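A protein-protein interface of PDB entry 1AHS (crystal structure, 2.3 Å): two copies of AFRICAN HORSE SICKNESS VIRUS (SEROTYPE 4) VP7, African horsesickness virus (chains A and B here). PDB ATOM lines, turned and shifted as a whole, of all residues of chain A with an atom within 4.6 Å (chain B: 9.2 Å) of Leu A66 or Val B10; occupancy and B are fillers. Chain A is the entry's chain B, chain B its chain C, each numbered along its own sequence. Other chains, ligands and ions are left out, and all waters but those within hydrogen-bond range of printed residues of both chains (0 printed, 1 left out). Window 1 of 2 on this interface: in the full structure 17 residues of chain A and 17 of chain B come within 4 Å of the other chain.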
ATOM      1  N   GLY A  14      -6.535 -20.125  16.979  1.00  0.00           N
ATOM      2  CA  GLY A  14      -6.962 -19.792  18.307  1.00  0.00           C
ATOM      3  C   GLY A  14      -8.296 -20.281  18.760  1.00  0.00           C
ATOM      4  O   GLY A  14      -8.742 -19.868  19.813  1.00  0.00           O
ATOM      5  N   GLU A  34      -0.842 -25.497  15.391  1.00  0.00           N
ATOM      6  CA  GLU A  34      -1.174 -25.212  16.780  1.00  0.00           C
ATOM      7  C   GLU A  34      -1.650 -26.490  17.440  1.00  0.00           C
ATOM      8  O   GLU A  34      -2.294 -27.299  16.793  1.00  0.00           O
ATOM      9  CB  GLU A  34      -2.339 -24.218  16.851  1.00  0.00           C
ATOM     10  CG  GLU A  34      -2.020 -22.783  16.430  1.00  0.00           C
ATOM     11  CD  GLU A  34      -3.197 -21.813  16.567  1.00  0.00           C
ATOM     12  OE1 GLU A  34      -4.345 -22.221  16.901  1.00  0.00           O
ATOM     13  OE2 GLU A  34      -2.977 -20.608  16.309  1.00  0.00           O
ATOM     14  N   ARG A  64       5.186 -20.768  21.214  1.00  0.00           N
ATOM     15  CA  ARG A  64       4.703 -19.864  22.233  1.00  0.00           C
ATOM     16  C   ARG A  64       3.250 -20.122  22.508  1.00  0.00           C
ATOM     17  O   ARG A  64       2.552 -20.707  21.691  1.00  0.00           O
ATOM     18  CB  ARG A  64       5.029 -18.383  21.984  1.00  0.00           C
ATOM     19  CG  ARG A  64       4.695 -17.812  20.687  1.00  0.00           C
ATOM     20  CD  ARG A  64       5.899 -17.864  19.764  1.00  0.00           C
ATOM     21  NE  ARG A  64       6.370 -16.558  19.298  1.00  0.00           N
ATOM     22  CZ  ARG A  64       6.209 -16.112  18.059  1.00  0.00           C
ATOM     23  NH1 ARG A  64       5.569 -16.854  17.146  1.00  0.00           N
ATOM     24  NH2 ARG A  64       6.723 -14.947  17.731  1.00  0.00           N
ATOM     25  N   PRO A  65       2.838 -19.901  23.744  1.00  0.00           N
ATOM     26  CA  PRO A  65       1.458 -20.107  24.162  1.00  0.00           C
ATOM     27  C   PRO A  65       0.625 -18.936  23.694  1.00  0.00           C
ATOM     28  O   PRO A  65       1.184 -17.900  23.344  1.00  0.00           O
ATOM     29  CB  PRO A  65       1.581 -20.132  25.683  1.00  0.00           C
ATOM     30  CG  PRO A  65       2.678 -19.163  25.948  1.00  0.00           C
ATOM     31  CD  PRO A  65       3.687 -19.520  24.886  1.00  0.00           C
ATOM     32  N   LEU A  66      -0.693 -19.109  23.602  1.00  0.00           N
ATOM     33  CA  LEU A  66      -1.511 -17.991  23.188  1.00  0.00           C
ATOM     34  C   LEU A  66      -2.015 -17.384  24.452  1.00  0.00           C
ATOM     35  O   LEU A  66      -2.689 -18.052  25.232  1.00  0.00           O
ATOM     36  CB  LEU A  66      -2.730 -18.406  22.363  1.00  0.00           C
ATOM     37  CG  LEU A  66      -2.723 -19.118  21.012  1.00  0.00           C
ATOM     38  CD1 LEU A  66      -3.718 -18.456  20.068  1.00  0.00           C
ATOM     39  CD2 LEU A  66      -1.356 -19.157  20.426  1.00  0.00           C
ATOM     40  N   ARG A  67      -1.662 -16.139  24.680  1.00  0.00           N
ATOM     41  CA  ARG A  67      -2.137 -15.447  25.844  1.00  0.00           C
ATOM     42  C   ARG A  67      -3.705 -15.450  25.863  1.00  0.00           C
ATOM     43  O   ARG A  67      -4.309 -15.670  26.914  1.00  0.00           O
ATOM     44  CB  ARG A  67      -1.526 -14.034  25.845  1.00  0.00           C
ATOM     45  CG  ARG A  67      -2.149 -13.055  26.840  1.00  0.00           C
ATOM     46  CD  ARG A  67      -1.835 -13.365  28.295  1.00  0.00           C
ATOM     47  NE  ARG A  67      -1.195 -12.200  28.914  1.00  0.00           N
ATOM     48  CZ  ARG A  67      -1.808 -11.356  29.739  1.00  0.00           C
ATOM     49  NH1 ARG A  67      -3.086 -11.560  30.062  1.00  0.00           N
ATOM     50  NH2 ARG A  67      -1.159 -10.283  30.197  1.00  0.00           N
ATOM     51  N   ILE A  68      -4.371 -15.127  24.745  1.00  0.00           N
ATOM     52  CA  ILE A  68      -5.836 -15.219  24.717  1.00  0.00           C
ATOM     53  C   ILE A  68      -6.284 -16.019  23.473  1.00  0.00           C
ATOM     54  O   ILE A  68      -5.652 -15.953  22.406  1.00  0.00           O
ATOM     55  CB  ILE A  68      -6.644 -13.838  24.799  1.00  0.00           C
ATOM     56  CG1 ILE A  68      -6.348 -13.005  23.622  1.00  0.00           C
ATOM     57  CG2 ILE A  68      -6.374 -12.999  26.048  1.00  0.00           C
ATOM     58  CD1 ILE A  68      -7.470 -13.097  22.703  1.00  0.00           C
ATOM     59  N   PHE A  69      -7.327 -16.829  23.633  1.00  0.00           N
ATOM     60  CA  PHE A  69      -7.873 -17.611  22.550  1.00  0.00           C
ATOM     61  C   PHE A  69      -9.350 -17.822  22.905  1.00  0.00           C
ATOM     62  O   PHE A  69      -9.820 -17.167  23.807  1.00  0.00           O
ATOM     63  CB  PHE A  69      -7.066 -18.915  22.366  1.00  0.00           C
ATOM     64  CG  PHE A  69      -7.162 -19.883  23.511  1.00  0.00           C
ATOM     65  CD1 PHE A  69      -6.262 -19.835  24.548  1.00  0.00           C
ATOM     66  CD2 PHE A  69      -8.122 -20.871  23.515  1.00  0.00           C
ATOM     67  CE1 PHE A  69      -6.323 -20.766  25.572  1.00  0.00           C
ATOM     68  CE2 PHE A  69      -8.184 -21.797  24.523  1.00  0.00           C
ATOM     69  CZ  PHE A  69      -7.274 -21.734  25.551  1.00  0.00           C
ATOM     70  N   SER A  79      -4.361 -19.089  28.174  1.00  0.00           N
ATOM     71  CA  SER A  79      -3.560 -20.293  28.309  1.00  0.00           C
ATOM     72  C   SER A  79      -3.010 -20.406  29.726  1.00  0.00           C
ATOM     73  O   SER A  79      -2.621 -19.386  30.365  1.00  0.00           O
ATOM     74  CB  SER A  79      -2.376 -20.240  27.325  1.00  0.00           C
ATOM     75  OG  SER A  79      -2.728 -20.757  26.062  1.00  0.00           O
ATOM     76  N   ILE A 117      -3.417 -23.363  24.228  1.00  0.00           N
ATOM     77  CA  ILE A 117      -3.173 -23.647  22.813  1.00  0.00           C
ATOM     78  C   ILE A 117      -1.733 -23.211  22.576  1.00  0.00           C
ATOM     79  O   ILE A 117      -1.354 -22.136  23.033  1.00  0.00           O
ATOM     80  CB  ILE A 117      -4.056 -22.859  21.843  1.00  0.00           C
ATOM     81  CG1 ILE A 117      -5.512 -23.246  21.967  1.00  0.00           C
ATOM     82  CG2 ILE A 117      -3.712 -23.231  20.414  1.00  0.00           C
ATOM     83  CD1 ILE A 117      -6.345 -22.515  20.983  1.00  0.00           C
ATOM     84  N   GLN A 119       1.360 -22.576  19.729  1.00  0.00           N
ATOM     85  CA  GLN A 119       1.605 -22.304  18.332  1.00  0.00           C
ATOM     86  C   GLN A 119       3.057 -22.618  17.987  1.00  0.00           C
ATOM     87  O   GLN A 119       3.931 -22.269  18.767  1.00  0.00           O
ATOM     88  CB  GLN A 119       1.339 -20.821  18.085  1.00  0.00           C
ATOM     89  CG  GLN A 119       1.766 -20.365  16.734  1.00  0.00           C
ATOM     90  CD  GLN A 119       1.567 -18.890  16.489  1.00  0.00           C
ATOM     91  OE1 GLN A 119       0.428 -18.437  16.313  1.00  0.00           O
ATOM     92  NE2 GLN A 119       2.680 -18.136  16.403  1.00  0.00           N
ATOM     93  N   TYR B   4       9.363 -10.364  15.358  1.00  0.00           N
ATOM     94  CA  TYR B   4       8.632 -10.714  16.548  1.00  0.00           C
ATOM     95  C   TYR B   4       8.768 -12.162  16.954  1.00  0.00           C
ATOM     96  O   TYR B   4       7.994 -12.700  17.752  1.00  0.00           O
ATOM     97  CB  TYR B   4       7.187 -10.268  16.396  1.00  0.00           C
ATOM     98  CG  TYR B   4       7.064  -8.823  15.942  1.00  0.00           C
ATOM     99  CD1 TYR B   4       7.946  -7.861  16.406  1.00  0.00           C
ATOM    100  CD2 TYR B   4       6.142  -8.453  14.981  1.00  0.00           C
ATOM    101  CE1 TYR B   4       7.931  -6.577  15.916  1.00  0.00           C
ATOM    102  CE2 TYR B   4       6.116  -7.174  14.475  1.00  0.00           C
ATOM    103  CZ  TYR B   4       7.023  -6.238  14.947  1.00  0.00           C
ATOM    104  OH  TYR B   4       7.056  -4.964  14.416  1.00  0.00           O
ATOM    105  N   ALA B   5       9.711 -12.837  16.329  1.00  0.00           N
ATOM    106  CA  ALA B   5      10.011 -14.205  16.726  1.00  0.00           C
ATOM    107  C   ALA B   5      10.795 -13.838  17.980  1.00  0.00           C
ATOM    108  O   ALA B   5      11.642 -12.937  17.950  1.00  0.00           O
ATOM    109  CB  ALA B   5      10.930 -14.818  15.716  1.00  0.00           C
ATOM    110  N   GLY B   6      10.542 -14.451  19.104  1.00  0.00           N
ATOM    111  CA  GLY B   6      11.317 -13.974  20.229  1.00  0.00           C
ATOM    112  C   GLY B   6      10.322 -13.472  21.212  1.00  0.00           C
ATOM    113  O   GLY B   6      10.591 -13.403  22.389  1.00  0.00           O
ATOM    114  N   ALA B   7       9.152 -13.117  20.711  1.00  0.00           N
ATOM    115  CA  ALA B   7       8.079 -12.672  21.561  1.00  0.00           C
ATOM    116  C   ALA B   7       7.801 -13.963  22.253  1.00  0.00           C
ATOM    117  O   ALA B   7       7.797 -14.998  21.592  1.00  0.00           O
ATOM    118  CB  ALA B   7       6.892 -12.289  20.715  1.00  0.00           C
ATOM    119  N   VAL B   8       7.513 -13.916  23.549  1.00  0.00           N
ATOM    120  CA  VAL B   8       7.241 -15.130  24.332  1.00  0.00           C
ATOM    121  C   VAL B   8       5.804 -15.644  24.415  1.00  0.00           C
ATOM    122  O   VAL B   8       5.525 -16.646  25.091  1.00  0.00           O
ATOM    123  CB  VAL B   8       7.810 -14.997  25.749  1.00  0.00           C
ATOM    124  CG1 VAL B   8       9.260 -14.513  25.674  1.00  0.00           C
ATOM    125  CG2 VAL B   8       7.001 -14.017  26.553  1.00  0.00           C
ATOM    126  N   GLU B   9       4.886 -14.924  23.783  1.00  0.00           N
ATOM    127  CA  GLU B   9       3.494 -15.316  23.729  1.00  0.00           C
ATOM    128  C   GLU B   9       2.851 -14.550  22.601  1.00  0.00           C
ATOM    129  O   GLU B   9       3.367 -13.527  22.143  1.00  0.00           O
ATOM    130  CB  GLU B   9       2.770 -15.101  25.064  1.00  0.00           C
ATOM    131  CG  GLU B   9       2.700 -13.666  25.540  1.00  0.00           C
ATOM    132  CD  GLU B   9       1.978 -13.504  26.864  1.00  0.00           C
ATOM    133  OE1 GLU B   9       2.055 -14.402  27.721  1.00  0.00           O
ATOM    134  OE2 GLU B   9       1.307 -12.464  27.041  1.00  0.00           O
ATOM    135  N   VAL B  10       1.795 -15.128  22.060  1.00  0.00           N
ATOM    136  CA  VAL B  10       1.089 -14.496  20.983  1.00  0.00           C
ATOM    137  C   VAL B  10      -0.367 -14.599  21.402  1.00  0.00           C
ATOM    138  O   VAL B  10      -0.684 -15.135  22.477  1.00  0.00           O
ATOM    139  CB  VAL B  10       1.341 -15.246  19.615  1.00  0.00           C
ATOM    140  CG1 VAL B  10       2.757 -15.072  19.189  1.00  0.00           C
ATOM    141  CG2 VAL B  10       1.037 -16.722  19.720  1.00  0.00           C
ATOM    142  N   GLN B  11      -1.253 -14.035  20.592  1.00  0.00           N
ATOM    143  CA  GLN B  11      -2.670 -14.137  20.871  1.00  0.00           C
ATOM    144  C   GLN B  11      -3.462 -14.327  19.589  1.00  0.00           C
ATOM    145  O   GLN B  11      -2.911 -14.215  18.501  1.00  0.00           O
ATOM    146  CB  GLN B  11      -3.144 -12.928  21.648  1.00  0.00           C
ATOM    147  CG  GLN B  11      -2.657 -11.646  21.100  1.00  0.00           C
ATOM    148  CD  GLN B  11      -2.871 -10.512  22.064  1.00  0.00           C
ATOM    149  OE1 GLN B  11      -3.864  -9.830  21.974  1.00  0.00           O
ATOM    150  NE2 GLN B  11      -1.941 -10.306  22.988  1.00  0.00           N
ATOM    151  N   GLN B  12      -4.715 -14.762  19.728  1.00  0.00           N
ATOM    152  CA  GLN B  12      -5.595 -14.960  18.584  1.00  0.00           C
ATOM    153  C   GLN B  12      -5.828 -13.657  17.848  1.00  0.00           C
ATOM    154  O   GLN B  12      -6.262 -12.676  18.439  1.00  0.00           O
ATOM    155  CB  GLN B  12      -6.961 -15.487  19.032  1.00  0.00           C
ATOM    156  CG  GLN B  12      -7.900 -15.689  17.858  1.00  0.00           C
ATOM    157  CD  GLN B  12      -9.257 -16.139  18.266  1.00  0.00           C
ATOM    158  OE1 GLN B  12      -9.726 -15.816  19.342  1.00  0.00           O
ATOM    159  NE2 GLN B  12      -9.916 -16.877  17.398  1.00  0.00           N
ATOM    160  N   SER B  13      -5.610 -13.656  16.546  1.00  0.00           N
ATOM    161  CA  SER B  13      -5.846 -12.459  15.766  1.00  0.00           C
ATOM    162  C   SER B  13      -7.304 -12.046  15.790  1.00  0.00           C
ATOM    163  O   SER B  13      -8.192 -12.885  15.762  1.00  0.00           O
ATOM    164  CB  SER B  13      -5.462 -12.707  14.326  1.00  0.00           C
ATOM    165  OG  SER B  13      -5.969 -11.698  13.481  1.00  0.00           O
ATOM    166  N   ARG B  15      -9.289 -10.717  18.134  1.00  0.00           N
ATOM    167  CA  ARG B  15     -10.110 -10.892  19.328  1.00  0.00           C
ATOM    168  C   ARG B  15      -9.769  -9.763  20.243  1.00  0.00           C
ATOM    169  O   ARG B  15      -8.710  -9.733  20.812  1.00  0.00           O
ATOM    170  CB  ARG B  15      -9.825 -12.230  20.018  1.00  0.00           C
ATOM    171  CG  ARG B  15     -10.517 -12.401  21.320  1.00  0.00           C
ATOM    172  CD  ARG B  15     -10.675 -13.859  21.694  1.00  0.00           C
ATOM    173  NE  ARG B  15     -11.576 -14.538  20.800  1.00  0.00           N
ATOM    174  CZ  ARG B  15     -12.842 -14.815  21.086  1.00  0.00           C
ATOM    175  NH1 ARG B  15     -13.347 -14.478  22.252  1.00  0.00           N
ATOM    176  NH2 ARG B  15     -13.609 -15.420  20.200  1.00  0.00           N
ATOM    177  N   TYR B  17      -9.005  -7.360  23.060  1.00  0.00           N
ATOM    178  CA  TYR B  17      -8.503  -7.595  24.434  1.00  0.00           C
ATOM    179  C   TYR B  17      -7.810  -6.332  24.942  1.00  0.00           C
ATOM    180  O   TYR B  17      -6.726  -6.021  24.485  1.00  0.00           O
ATOM    181  CB  TYR B  17      -7.450  -8.698  24.444  1.00  0.00           C
ATOM    182  CG  TYR B  17      -6.955  -9.073  25.810  1.00  0.00           C
ATOM    183  CD1 TYR B  17      -7.810  -9.653  26.741  1.00  0.00           C
ATOM    184  CD2 TYR B  17      -5.619  -8.896  26.158  1.00  0.00           C
ATOM    185  CE1 TYR B  17      -7.343 -10.061  28.001  1.00  0.00           C
ATOM    186  CE2 TYR B  17      -5.133  -9.291  27.410  1.00  0.00           C
ATOM    187  CZ  TYR B  17      -5.999  -9.872  28.329  1.00  0.00           C
ATOM    188  OH  TYR B  17      -5.536 -10.249  29.576  1.00  0.00           O
ATOM    189  N   ARG B  24      -4.103  -1.556  23.670  1.00  0.00           N
ATOM    190  CA  ARG B  24      -3.190  -2.637  24.073  1.00  0.00           C
ATOM    191  C   ARG B  24      -2.673  -3.303  22.798  1.00  0.00           C
ATOM    192  O   ARG B  24      -3.373  -3.325  21.805  1.00  0.00           O
ATOM    193  CB  ARG B  24      -3.812  -3.688  24.996  1.00  0.00           C
ATOM    194  CG  ARG B  24      -2.777  -4.775  25.452  1.00  0.00           C
ATOM    195  CD  ARG B  24      -3.381  -5.876  26.340  1.00  0.00           C
ATOM    196  NE  ARG B  24      -2.474  -6.957  26.772  1.00  0.00           N
ATOM    197  CZ  ARG B  24      -1.839  -7.786  25.949  1.00  0.00           C
ATOM    198  NH1 ARG B  24      -2.000  -7.658  24.648  1.00  0.00           N
ATOM    199  NH2 ARG B  24      -1.059  -8.757  26.427  1.00  0.00           N
ATOM    200  N   GLY B  25      -1.406  -3.711  22.802  1.00  0.00           N
ATOM    201  CA  GLY B  25      -0.781  -4.389  21.676  1.00  0.00           C
ATOM    202  C   GLY B  25      -0.335  -5.805  22.058  1.00  0.00           C
ATOM    203  O   GLY B  25      -0.129  -6.125  23.246  1.00  0.00           O
ATOM    204  N   GLY B  26      -0.213  -6.663  21.046  1.00  0.00           N
ATOM    205  CA  GLY B  26       0.203  -8.049  21.236  1.00  0.00           C
ATOM    206  C   GLY B  26       0.713  -8.567  19.911  1.00  0.00           C
ATOM    207  O   GLY B  26       0.497  -7.940  18.883  1.00  0.00           O
ATOM    208  N   TYR B  27       1.383  -9.704  19.907  1.00  0.00           N
ATOM    209  CA  TYR B  27       1.885 -10.203  18.653  1.00  0.00           C
ATOM    210  C   TYR B  27       1.057 -11.318  18.159  1.00  0.00           C
ATOM    211  O   TYR B  27       0.557 -12.104  18.938  1.00  0.00           O
ATOM    212  CB  TYR B  27       3.301 -10.683  18.810  1.00  0.00           C
ATOM    213  CG  TYR B  27       4.227  -9.571  19.189  1.00  0.00           C
ATOM    214  CD1 TYR B  27       4.570  -8.591  18.270  1.00  0.00           C
ATOM    215  CD2 TYR B  27       4.729  -9.467  20.480  1.00  0.00           C
ATOM    216  CE1 TYR B  27       5.409  -7.509  18.632  1.00  0.00           C
ATOM    217  CE2 TYR B  27       5.566  -8.391  20.857  1.00  0.00           C
ATOM    218  CZ  TYR B  27       5.903  -7.412  19.935  1.00  0.00           C
ATOM    219  OH  TYR B  27       6.692  -6.330  20.318  1.00  0.00           O
ATOM    220  N   ILE B  28       0.968 -11.431  16.845  1.00  0.00           N
ATOM    221  CA  ILE B  28       0.192 -12.496  16.210  1.00  0.00           C
ATOM    222  C   ILE B  28       1.112 -13.656  15.755  1.00  0.00           C
ATOM    223  O   ILE B  28       0.827 -14.823  16.001  1.00  0.00           O
ATOM    224  CB  ILE B  28      -0.670 -11.907  15.066  1.00  0.00           C
ATOM    225  CG1 ILE B  28      -1.683 -10.902  15.643  1.00  0.00           C
ATOM    226  CG2 ILE B  28      -1.381 -12.996  14.314  1.00  0.00           C
ATOM    227  CD1 ILE B  28      -2.450 -11.403  16.881  1.00  0.00           C
ATOM    228  N   ASN B  29       2.229 -13.311  15.128  1.00  0.00           N
ATOM    229  CA  ASN B  29       3.251 -14.243  14.693  1.00  0.00           C
ATOM    230  C   ASN B  29       4.489 -13.407  14.493  1.00  0.00           C
ATOM    231  O   ASN B  29       4.517 -12.230  14.849  1.00  0.00           O
ATOM    232  CB  ASN B  29       2.894 -14.942  13.407  1.00  0.00           C
ATOM    233  CG  ASN B  29       2.663 -14.000  12.278  1.00  0.00           C
ATOM    234  OD1 ASN B  29       3.375 -13.041  12.087  1.00  0.00           O
ATOM    235  ND2 ASN B  29       1.667 -14.289  11.504  1.00  0.00           N
ATOM    236  N   SER B  30       5.481 -13.962  13.825  1.00  0.00           N
ATOM    237  CA  SER B  30       6.742 -13.257  13.627  1.00  0.00           C
ATOM    238  C   SER B  30       6.763 -11.938  12.916  1.00  0.00           C
ATOM    239  O   SER B  30       7.717 -11.197  13.107  1.00  0.00           O
ATOM    240  CB  SER B  30       7.747 -14.175  12.959  1.00  0.00           C
ATOM    241  OG  SER B  30       8.029 -15.240  13.836  1.00  0.00           O
ATOM    242  N   ASN B  31       5.744 -11.618  12.122  1.00  0.00           N
ATOM    243  CA  ASN B  31       5.737 -10.370  11.359  1.00  0.00           C
ATOM    244  C   ASN B  31       4.563  -9.539  11.586  1.00  0.00           C
ATOM    245  O   ASN B  31       4.414  -8.537  10.927  1.00  0.00           O
ATOM    246  CB  ASN B  31       5.634 -10.640   9.881  1.00  0.00           C
ATOM    247  CG  ASN B  31       6.567 -11.660   9.441  1.00  0.00           C
ATOM    248  OD1 ASN B  31       6.201 -12.833   9.299  1.00  0.00           O
ATOM    249  ND2 ASN B  31       7.819 -11.258   9.243  1.00  0.00           N
ATOM    250  N   ILE B  32       3.674  -9.971  12.439  1.00  0.00           N
ATOM    251  CA  ILE B  32       2.487  -9.202  12.592  1.00  0.00           C
ATOM    252  C   ILE B  32       2.159  -8.884  14.024  1.00  0.00           C
ATOM    253  O   ILE B  32       2.178  -9.772  14.898  1.00  0.00           O
ATOM    254  CB  ILE B  32       1.310  -9.953  11.943  1.00  0.00           C
ATOM    255  CG1 ILE B  32       1.493 -10.010  10.430  1.00  0.00           C
ATOM    256  CG2 ILE B  32       0.026  -9.261  12.256  1.00  0.00           C
ATOM    257  CD1 ILE B  32       0.448 -10.847   9.754  1.00  0.00           C
ATOM    258  N   ALA B  33       1.783  -7.620  14.237  1.00  0.00           N
ATOM    259  CA  ALA B  33       1.397  -7.132  15.542  1.00  0.00           C
ATOM    260  C   ALA B  33       0.006  -6.517  15.349  1.00  0.00           C
ATOM    261  O   ALA B  33      -0.300  -6.030  14.274  1.00  0.00           O
ATOM    262  CB  ALA B  33       2.386  -6.092  15.987  1.00  0.00           C
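The backbone carbonyl oxygen (O) of Pro A65 is in hydrogen-bond range of the backbone NH (N) of Val B10 (3.1 Å). NH2 of Arg A64 sits at hydrogen-bond distance from O of Tyr B4 (2.6 Å). The guanidinium group (NE) of Arg A67 lies within salt-bridge range of the side-chain carboxylate (OE2) of Glu B9 (3.1 Å). NE of Arg A64 lies within hydrogen-bond range of O of Ala B7, 3.1 Å away. The guanidinium group (NH1) of Arg A67 sits at hydrogen-bond distance from the side-chain hydroxyl (OH) of Tyr B17, 2.8 Å away. The backbone NH (N) of Arg A67 is in hydrogen-bond range of the backbone carbonyl oxygen (O) of Val B10 (2.6 Å). The backbone carbonyl oxygen of Ile A68 lies within hydrogen-bond range of the backbone NH of Gln B12.
O of Arg A64 is in hydrogen-bond range of N of Gln A119, 3.0 Å away. The backbone NH (N) of Leu A66 lies within hydrogen-bond range of the backbone carbonyl oxygen (O) of Ile A117 (3.2 Å). O of Ser B30 lies within hydrogen-bond range of N of Tyr B4 (2.9 Å). NE2 of Gln B11 sits close to NH1 of Arg B24 (3.1 Å). The backbone NH (N) of Gln B11 is in hydrogen-bond range of the backbone carbonyl oxygen (O) of Tyr B27. NE of Arg B15 sits at hydrogen-bond distance from OE1 of Gln B12 (2.7 Å).
Among the printed residues, merely in contact across the chains: Arg A64 with Ala B5 (3.5 Å), Arg A64 with Val B8 (3.6 Å), Arg A64 with Glu B9 (3.8 Å), Arg A64 with Val B10 (3.7 Å), Pro A65 with Val B8 (3.4 Å), Pro A65 with Glu B9 (3.5 Å), Leu A66 with Val B10 (3.1 Å), Leu A66 with Gln B12 (3.8 Å), Ile A68 with Gln B11 (3.8 Å), Ile A68 with Arg B15 (3.4 Å), Ile A68 with Tyr B17 (3.7 Å), Gln A119 with Val B10 (3.9 Å) and Gln A119 with Ile B28 (3.6 Å).
Of chain A, only Arg A64 (3.7 Å), Pro A65 (3.1 Å), Leu A66 (3.1 Å), Arg A67 (2.6 Å) and Gln A119 (3.9 Å) come within 4 Å of Val B10. Pro A65 touches just these residues of chain B: Val B8 (3.4 Å), Glu B9 (3.5 Å) and Val B10 (3.1 Å). No residue of chain B comes within 4 Å of Ile A117. Of the printed residues of chain A, Arg B15 touches Ile A68. Printed residues of chain B within 4 Å of Ile A68: Gln B11, Gln B12, Arg B15 and Tyr B17. Of the printed residues of chain A, Gln B11 touches Ile A68 (3.8 Å). Of the printed residues of chain B, Gln A119 touches Val B10 (3.9 Å) and Ile B28 (3.6 Å). Printed residues of chain A within 4 Å of Tyr B4: Arg A64. Gly A14 touches none of the printed residues of chain B. Tyr B27 touches none of the printed residues of chain A. The nearest residue of chain A that does not touch Val B10 is Ile A68 (4.3 Å).
Hydrophobic or aromatic side chains of chain B that line the printed part of chain A: Ala B7, Val B10 and Tyr B17. Of the 11 printed residues of chain A, 6 touch a printed residue of chain B. Printed residues of chain A that touch a printed residue of chain B: Arg A64, Pro A65, Leu A66, Arg A67, Ile A68 and Gln A119. Hydrophobic or aromatic side chains of chain A within 4 Å of the printed part of chain B: Pro A65, Leu A66 and Ile A68. Among the printed residues, Asp or Glu carboxylates within 4 Å of a Lys or Arg side-chain nitrogen of the other chain: Arg A67 with Glu B9.
No position is printed for both chains.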
